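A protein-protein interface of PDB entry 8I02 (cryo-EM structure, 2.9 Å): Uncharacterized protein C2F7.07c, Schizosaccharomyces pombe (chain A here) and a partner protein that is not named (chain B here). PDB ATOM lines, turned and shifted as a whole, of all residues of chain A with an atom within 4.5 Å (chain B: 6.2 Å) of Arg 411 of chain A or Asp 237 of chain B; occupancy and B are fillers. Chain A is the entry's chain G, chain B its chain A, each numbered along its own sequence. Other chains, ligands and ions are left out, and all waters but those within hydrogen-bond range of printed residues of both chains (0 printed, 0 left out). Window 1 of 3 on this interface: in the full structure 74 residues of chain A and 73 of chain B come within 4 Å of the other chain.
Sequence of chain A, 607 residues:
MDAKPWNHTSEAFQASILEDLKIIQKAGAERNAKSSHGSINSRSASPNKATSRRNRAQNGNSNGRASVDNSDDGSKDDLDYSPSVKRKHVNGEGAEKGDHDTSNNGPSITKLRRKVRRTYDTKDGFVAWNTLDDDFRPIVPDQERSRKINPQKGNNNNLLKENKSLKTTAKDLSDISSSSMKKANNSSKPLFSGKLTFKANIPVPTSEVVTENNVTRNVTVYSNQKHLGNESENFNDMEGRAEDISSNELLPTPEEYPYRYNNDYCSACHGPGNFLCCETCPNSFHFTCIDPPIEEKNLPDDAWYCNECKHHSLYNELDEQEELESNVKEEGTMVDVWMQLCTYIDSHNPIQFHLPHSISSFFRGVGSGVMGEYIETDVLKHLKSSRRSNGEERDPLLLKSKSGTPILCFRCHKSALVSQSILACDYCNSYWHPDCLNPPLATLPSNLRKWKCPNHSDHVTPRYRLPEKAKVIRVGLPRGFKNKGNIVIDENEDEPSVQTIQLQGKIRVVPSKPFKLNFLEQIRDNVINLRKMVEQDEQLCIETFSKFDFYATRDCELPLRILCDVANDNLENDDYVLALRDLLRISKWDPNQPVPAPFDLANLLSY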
ATOM      1  N   CYS A 409       7.913  -7.412   9.356  1.00  0.00           N
ATOM      2  CA  CYS A 409       8.345  -8.709   9.853  1.00  0.00           C
ATOM      3  C   CYS A 409       9.190  -8.541  11.108  1.00  0.00           C
ATOM      4  O   CYS A 409       9.855  -7.523  11.304  1.00  0.00           O
ATOM      5  CB  CYS A 409       9.140  -9.447   8.779  1.00  0.00           C
ATOM      6  SG  CYS A 409       9.670 -11.113   9.185  1.00  0.00           S
ATOM      7  N   PHE A 410       9.144  -9.549  11.978  1.00  0.00           N
ATOM      8  CA  PHE A 410       9.931  -9.530  13.203  1.00  0.00           C
ATOM      9  C   PHE A 410      11.372  -9.957  12.973  1.00  0.00           C
ATOM     10  O   PHE A 410      12.224  -9.706  13.824  1.00  0.00           O
ATOM     11  CB  PHE A 410       9.270 -10.429  14.250  1.00  0.00           C
ATOM     12  CG  PHE A 410       9.731 -10.180  15.661  1.00  0.00           C
ATOM     13  CD1 PHE A 410      10.865 -10.803  16.155  1.00  0.00           C
ATOM     14  CD2 PHE A 410       9.014  -9.360  16.502  1.00  0.00           C
ATOM     15  CE1 PHE A 410      11.291 -10.584  17.439  1.00  0.00           C
ATOM     16  CE2 PHE A 410       9.434  -9.146  17.792  1.00  0.00           C
ATOM     17  CZ  PHE A 410      10.573  -9.760  18.260  1.00  0.00           C
ATOM     18  N   ARG A 411      11.675 -10.569  11.839  1.00  0.00           N
ATOM     19  CA  ARG A 411      12.996 -11.130  11.613  1.00  0.00           C
ATOM     20  C   ARG A 411      13.867 -10.295  10.686  1.00  0.00           C
ATOM     21  O   ARG A 411      15.029 -10.035  11.002  1.00  0.00           O
ATOM     22  CB  ARG A 411      12.871 -12.547  11.057  1.00  0.00           C
ATOM     23  CG  ARG A 411      14.207 -13.112  10.693  1.00  0.00           C
ATOM     24  CD  ARG A 411      14.116 -14.542  10.332  1.00  0.00           C
ATOM     25  NE  ARG A 411      15.419 -15.183  10.331  1.00  0.00           N
ATOM     26  CZ  ARG A 411      15.613 -16.444   9.975  1.00  0.00           C
ATOM     27  NH1 ARG A 411      14.584 -17.181   9.595  1.00  0.00           N
ATOM     28  NH2 ARG A 411      16.828 -16.971   9.998  1.00  0.00           N
ATOM     29  N   CYS A 412      13.354  -9.882   9.534  1.00  0.00           N
ATOM     30  CA  CYS A 412      14.123  -9.084   8.596  1.00  0.00           C
ATOM     31  C   CYS A 412      13.747  -7.615   8.632  1.00  0.00           C
ATOM     32  O   CYS A 412      14.482  -6.795   8.081  1.00  0.00           O
ATOM     33  CB  CYS A 412      13.976  -9.630   7.168  1.00  0.00           C
ATOM     34  SG  CYS A 412      12.298  -9.940   6.599  1.00  0.00           S
ATOM     35  N   HIS A 413      12.639  -7.272   9.277  1.00  0.00           N
ATOM     36  CA  HIS A 413      12.139  -5.928   9.538  1.00  0.00           C
ATOM     37  C   HIS A 413      11.437  -5.292   8.342  1.00  0.00           C
ATOM     38  O   HIS A 413      11.040  -4.135   8.443  1.00  0.00           O
ATOM     39  CB  HIS A 413      13.238  -4.977  10.030  1.00  0.00           C
ATOM     40  CG  HIS A 413      13.898  -5.426  11.296  1.00  0.00           C
ATOM     41  ND1 HIS A 413      13.305  -5.294  12.530  1.00  0.00           N
ATOM     42  CD2 HIS A 413      15.099  -6.009  11.515  1.00  0.00           C
ATOM     43  CE1 HIS A 413      14.110  -5.779  13.455  1.00  0.00           C
ATOM     44  NE2 HIS A 413      15.204  -6.221  12.865  1.00  0.00           N
ATOM     45  N   TRP A 432       5.123 -11.938  10.813  1.00  0.00           N
ATOM     46  CA  TRP A 432       6.186 -12.738  10.232  1.00  0.00           C
ATOM     47  C   TRP A 432       5.886 -13.022   8.769  1.00  0.00           C
ATOM     48  O   TRP A 432       4.727 -13.130   8.373  1.00  0.00           O
ATOM     49  CB  TRP A 432       6.359 -14.070  10.985  1.00  0.00           C
ATOM     50  CG  TRP A 432       6.821 -13.955  12.405  1.00  0.00           C
ATOM     51  CD1 TRP A 432       6.082 -13.567  13.484  1.00  0.00           C
ATOM     52  CD2 TRP A 432       8.122 -14.250  12.901  1.00  0.00           C
ATOM     53  NE1 TRP A 432       6.847 -13.597  14.613  1.00  0.00           N
ATOM     54  CE2 TRP A 432       8.105 -14.014  14.283  1.00  0.00           C
ATOM     55  CE3 TRP A 432       9.300 -14.698  12.310  1.00  0.00           C
ATOM     56  CZ2 TRP A 432       9.216 -14.200  15.078  1.00  0.00           C
ATOM     57  CZ3 TRP A 432      10.399 -14.882  13.102  1.00  0.00           C
ATOM     58  CH2 TRP A 432      10.353 -14.627  14.473  1.00  0.00           C
ATOM     59  N   CYS A 436      10.298 -16.667   6.312  1.00  0.00           N
ATOM     60  CA  CYS A 436      11.313 -16.418   7.325  1.00  0.00           C
ATOM     61  C   CYS A 436      11.271 -17.398   8.488  1.00  0.00           C
ATOM     62  O   CYS A 436      12.316 -17.644   9.095  1.00  0.00           O
ATOM     63  CB  CYS A 436      11.178 -14.994   7.869  1.00  0.00           C
ATOM     64  SG  CYS A 436      11.963 -13.722   6.848  1.00  0.00           S
ATOM     65  N   SER B 227      20.460 -18.944   2.985  1.00  0.00           N
ATOM     66  CA  SER B 227      19.437 -17.926   2.817  1.00  0.00           C
ATOM     67  C   SER B 227      20.003 -16.538   3.136  1.00  0.00           C
ATOM     68  O   SER B 227      21.113 -16.392   3.643  1.00  0.00           O
ATOM     69  CB  SER B 227      18.241 -18.231   3.715  1.00  0.00           C
ATOM     70  OG  SER B 227      17.055 -17.689   3.185  1.00  0.00           O
ATOM     71  N   SER B 228      19.229 -15.500   2.821  1.00  0.00           N
ATOM     72  CA  SER B 228      19.688 -14.142   3.073  1.00  0.00           C
ATOM     73  C   SER B 228      18.641 -13.205   3.646  1.00  0.00           C
ATOM     74  O   SER B 228      19.010 -12.115   4.078  1.00  0.00           O
ATOM     75  CB  SER B 228      20.253 -13.532   1.791  1.00  0.00           C
ATOM     76  OG  SER B 228      21.263 -14.371   1.274  1.00  0.00           O
ATOM     77  N   GLN B 229      17.367 -13.566   3.649  1.00  0.00           N
ATOM     78  CA  GLN B 229      16.322 -12.809   4.337  1.00  0.00           C
ATOM     79  C   GLN B 229      16.172 -11.401   3.778  1.00  0.00           C
ATOM     80  O   GLN B 229      16.075 -10.431   4.523  1.00  0.00           O
ATOM     81  CB  GLN B 229      16.565 -12.764   5.846  1.00  0.00           C
ATOM     82  CG  GLN B 229      16.371 -14.081   6.557  1.00  0.00           C
ATOM     83  CD  GLN B 229      17.641 -14.892   6.597  1.00  0.00           C
ATOM     84  OE1 GLN B 229      18.728 -14.354   6.478  1.00  0.00           O
ATOM     85  NE2 GLN B 229      17.508 -16.193   6.766  1.00  0.00           N
ATOM     86  N   ILE B 235      24.026 -11.795   2.555  1.00  0.00           N
ATOM     87  CA  ILE B 235      24.781 -12.363   3.667  1.00  0.00           C
ATOM     88  C   ILE B 235      23.792 -12.854   4.714  1.00  0.00           C
ATOM     89  O   ILE B 235      22.942 -12.088   5.180  1.00  0.00           O
ATOM     90  CB  ILE B 235      25.773 -11.352   4.274  1.00  0.00           C
ATOM     91  CG1 ILE B 235      26.870 -11.015   3.268  1.00  0.00           C
ATOM     92  CG2 ILE B 235      26.420 -11.927   5.497  1.00  0.00           C
ATOM     93  CD1 ILE B 235      27.526  -9.716   3.518  1.00  0.00           C
ATOM     94  N   SER B 236      23.896 -14.137   5.066  1.00  0.00           N
ATOM     95  CA  SER B 236      22.993 -14.759   6.025  1.00  0.00           C
ATOM     96  C   SER B 236      23.194 -14.179   7.414  1.00  0.00           C
ATOM     97  O   SER B 236      24.325 -14.004   7.869  1.00  0.00           O
ATOM     98  CB  SER B 236      23.230 -16.264   6.059  1.00  0.00           C
ATOM     99  OG  SER B 236      22.069 -16.967   6.454  1.00  0.00           O
ATOM    100  N   ASP B 237      22.094 -13.904   8.103  1.00  0.00           N
ATOM    101  CA  ASP B 237      22.173 -13.338   9.442  1.00  0.00           C
ATOM    102  C   ASP B 237      22.514 -14.367  10.503  1.00  0.00           C
ATOM    103  O   ASP B 237      22.454 -14.045  11.690  1.00  0.00           O
ATOM    104  CB  ASP B 237      20.871 -12.625   9.805  1.00  0.00           C
ATOM    105  CG  ASP B 237      19.717 -13.570   9.999  1.00  0.00           C
ATOM    106  OD1 ASP B 237      19.794 -14.730   9.559  1.00  0.00           O
ATOM    107  OD2 ASP B 237      18.705 -13.142  10.582  1.00  0.00           O
ATOM    108  N   LEU B 238      22.840 -15.593  10.117  1.00  0.00           N
ATOM    109  CA  LEU B 238      23.378 -16.571  11.046  1.00  0.00           C
ATOM    110  C   LEU B 238      24.878 -16.450  11.205  1.00  0.00           C
ATOM    111  O   LEU B 238      25.428 -16.979  12.170  1.00  0.00           O
ATOM    112  CB  LEU B 238      23.057 -17.993  10.583  1.00  0.00           C
ATOM    113  CG  LEU B 238      21.908 -18.761  11.231  1.00  0.00           C
ATOM    114  CD1 LEU B 238      20.570 -18.129  10.924  1.00  0.00           C
ATOM    115  CD2 LEU B 238      21.953 -20.188  10.759  1.00  0.00           C
ATOM    116  N   LEU B 239      25.551 -15.782  10.272  1.00  0.00           N
ATOM    117  CA  LEU B 239      26.984 -15.569  10.341  1.00  0.00           C
ATOM    118  C   LEU B 239      27.356 -14.127  10.617  1.00  0.00           C
ATOM    119  O   LEU B 239      28.471 -13.870  11.068  1.00  0.00           O
ATOM    120  CB  LEU B 239      27.660 -16.000   9.032  1.00  0.00           C
ATOM    121  CG  LEU B 239      27.405 -17.371   8.422  1.00  0.00           C
ATOM    122  CD1 LEU B 239      26.281 -17.295   7.454  1.00  0.00           C
ATOM    123  CD2 LEU B 239      28.635 -17.807   7.703  1.00  0.00           C
ATOM    124  N   SER B 240      26.463 -13.185  10.346  1.00  0.00           N
ATOM    125  CA  SER B 240      26.757 -11.788  10.618  1.00  0.00           C
ATOM    126  C   SER B 240      26.596 -11.474  12.096  1.00  0.00           C
ATOM    127  O   SER B 240      27.501 -10.912  12.721  1.00  0.00           O
ATOM    128  CB  SER B 240      25.842 -10.893   9.792  1.00  0.00           C
ATOM    129  OG  SER B 240      25.670 -11.422   8.499  1.00  0.00           O
ATOM    130  N   GLN B 241      25.446 -11.836  12.667  1.00  0.00           N
ATOM    131  CA  GLN B 241      25.106 -11.504  14.041  1.00  0.00           C
ATOM    132  C   GLN B 241      25.863 -12.326  15.058  1.00  0.00           C
ATOM    133  O   GLN B 241      25.757 -12.037  16.252  1.00  0.00           O
ATOM    134  CB  GLN B 241      23.617 -11.702  14.273  1.00  0.00           C
ATOM    135  CG  GLN B 241      22.756 -11.165  13.181  1.00  0.00           C
ATOM    136  CD  GLN B 241      22.965  -9.688  12.958  1.00  0.00           C
ATOM    137  OE1 GLN B 241      22.366  -8.856  13.631  1.00  0.00           O
ATOM    138  NE2 GLN B 241      23.827  -9.351  12.006  1.00  0.00           N
ATOM    139  N   SER B 242      26.611 -13.337  14.629  1.00  0.00           N
ATOM    140  CA  SER B 242      27.182 -14.304  15.550  1.00  0.00           C
ATOM    141  C   SER B 242      28.610 -14.654  15.174  1.00  0.00           C
ATOM    142  O   SER B 242      29.000 -15.821  15.216  1.00  0.00           O
ATOM    143  CB  SER B 242      26.332 -15.569  15.596  1.00  0.00           C
ATOM    144  OG  SER B 242      26.839 -16.546  14.716  1.00  0.00           O
ATOM    145  N   PHE B 299      17.642 -17.447  19.422  1.00  0.00           N
ATOM    146  CA  PHE B 299      18.065 -16.644  18.281  1.00  0.00           C
ATOM    147  C   PHE B 299      16.920 -15.789  17.778  1.00  0.00           C
ATOM    148  O   PHE B 299      17.092 -14.601  17.506  1.00  0.00           O
ATOM    149  CB  PHE B 299      18.588 -17.551  17.173  1.00  0.00           C
ATOM    150  CG  PHE B 299      19.220 -16.822  16.020  1.00  0.00           C
ATOM    151  CD1 PHE B 299      18.631 -16.837  14.773  1.00  0.00           C
ATOM    152  CD2 PHE B 299      20.409 -16.141  16.177  1.00  0.00           C
ATOM    153  CE1 PHE B 299      19.206 -16.185  13.721  1.00  0.00           C
ATOM    154  CE2 PHE B 299      20.990 -15.487  15.116  1.00  0.00           C
ATOM    155  CZ  PHE B 299      20.388 -15.510  13.893  1.00  0.00           C
ATOM    156  N   LYS B 303      18.532 -11.456  18.101  1.00  0.00           N
ATOM    157  CA  LYS B 303      19.564 -11.546  17.079  1.00  0.00           C
ATOM    158  C   LYS B 303      19.779 -10.248  16.339  1.00  0.00           C
ATOM    159  O   LYS B 303      20.854 -10.062  15.763  1.00  0.00           O
ATOM    160  CB  LYS B 303      19.227 -12.639  16.059  1.00  0.00           C
ATOM    161  CG  LYS B 303      18.015 -12.337  15.205  1.00  0.00           C
ATOM    162  CD  LYS B 303      18.399 -12.017  13.784  1.00  0.00           C
ATOM    163  CE  LYS B 303      17.207 -11.521  13.009  1.00  0.00           C
ATOM    164  NZ  LYS B 303      17.602 -11.063  11.663  1.00  0.00           N
ATOM    165  N   SER B 304      18.807  -9.337  16.337  1.00  0.00           N
ATOM    166  CA  SER B 304      18.982  -8.034  15.720  1.00  0.00           C
ATOM    167  C   SER B 304      19.680  -7.113  16.701  1.00  0.00           C
ATOM    168  O   SER B 304      19.253  -5.976  16.923  1.00  0.00           O
ATOM    169  CB  SER B 304      17.634  -7.461  15.316  1.00  0.00           C
ATOM    170  OG  SER B 304      16.659  -7.822  16.271  1.00  0.00           O
ATOM    171  N   TYR B 327      21.618 -25.390  14.608  1.00  0.00           N
ATOM    172  CA  TYR B 327      20.485 -24.468  14.594  1.00  0.00           C
ATOM    173  C   TYR B 327      19.244 -25.089  13.967  1.00  0.00           C
ATOM    174  O   TYR B 327      18.129 -24.877  14.451  1.00  0.00           O
ATOM    175  CB  TYR B 327      20.856 -23.185  13.860  1.00  0.00           C
ATOM    176  CG  TYR B 327      19.679 -22.271  13.642  1.00  0.00           C
ATOM    177  CD1 TYR B 327      19.180 -22.039  12.379  1.00  0.00           C
ATOM    178  CD2 TYR B 327      19.059 -21.647  14.708  1.00  0.00           C
ATOM    179  CE1 TYR B 327      18.103 -21.217  12.185  1.00  0.00           C
ATOM    180  CE2 TYR B 327      17.983 -20.822  14.520  1.00  0.00           C
ATOM    181  CZ  TYR B 327      17.511 -20.611  13.259  1.00  0.00           C
ATOM    182  OH  TYR B 327      16.440 -19.784  13.070  1.00  0.00           O
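Among the printed residues, pairs that only touch across the chains: Cys 412 of chain A with Gln 229 of chain B (3.5 Å) and His 413 of chain A with Ser 304 of chain B (3.7 Å).
Of the 7 printed residues of chain A, 3 touch a printed residue of chain B. Printed residues of chain A that touch a printed residue of chain B: Arg 411, Cys 412 and His 413. Hydrophobic or aromatic side chains of chain A within 4 Å of the printed part of chain B: His 413. Of the 15 printed residues of chain B, 4 touch a printed residue of chain A. Printed residues of chain B that touch a printed residue of chain A: Gln 229, Asp 237, Lys 303 and Ser 304. Among the printed residues, 5 pairs touch across the chains. Among the printed residues, Asp or Glu carboxylates within 4 Å of a Lys or Arg side-chain nitrogen of the other chain: Arg 411 of chain A with Asp 237 of chain B.
Cys 409 of chain A touches none of the printed residues of chain B. Phe 410 of chain A touches none of the printed residues of chain B. Arg 411 of chain A touches three residues of chain B. Of the printed residues of chain B, Cys 412 of chain A touches Gln 229. Of the printed residues of chain B, His 413 of chain A touches Ser 304. Of the printed residues of chain A, Gln 229 of chain B touches Arg 411 and Cys 412. Of the printed residues of chain A, Lys 303 of chain B touches Arg 411 (2.8 Å). Of the printed residues of chain A, Ser 304 of chain B touches His 413.
The guanidinium group (NH2) of Arg 411 of chain A lies within salt-bridge range of the side-chain carboxylate (OD1) of Asp 237 of chain B, at 3.7 Å. The backbone carbonyl oxygen (O) of Arg 411 of chain A sits at hydrogen-bond distance from the side-chain amino group (NZ) of Lys 303 of chain B (2.8 Å). NE2 of Gln 229 of chain B lies close to NH2 of Arg 411 of chain A.
The side-chain amino group (NZ) of Lys 303 of chain B lies within salt-bridge range of the side-chain carboxylate (OD2) of Asp 237 of chain B (2.6 Å). OE1 of Gln 229 of chain B lies close to OD1 of Asp 237 of chain B, at 3.3 Å. N of Arg 411 of chain A lies close to SG of Cys 409 of chain A. O of Lys 303 of chain B sits close to OE1 of Gln 241 of chain B (2.9 Å).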
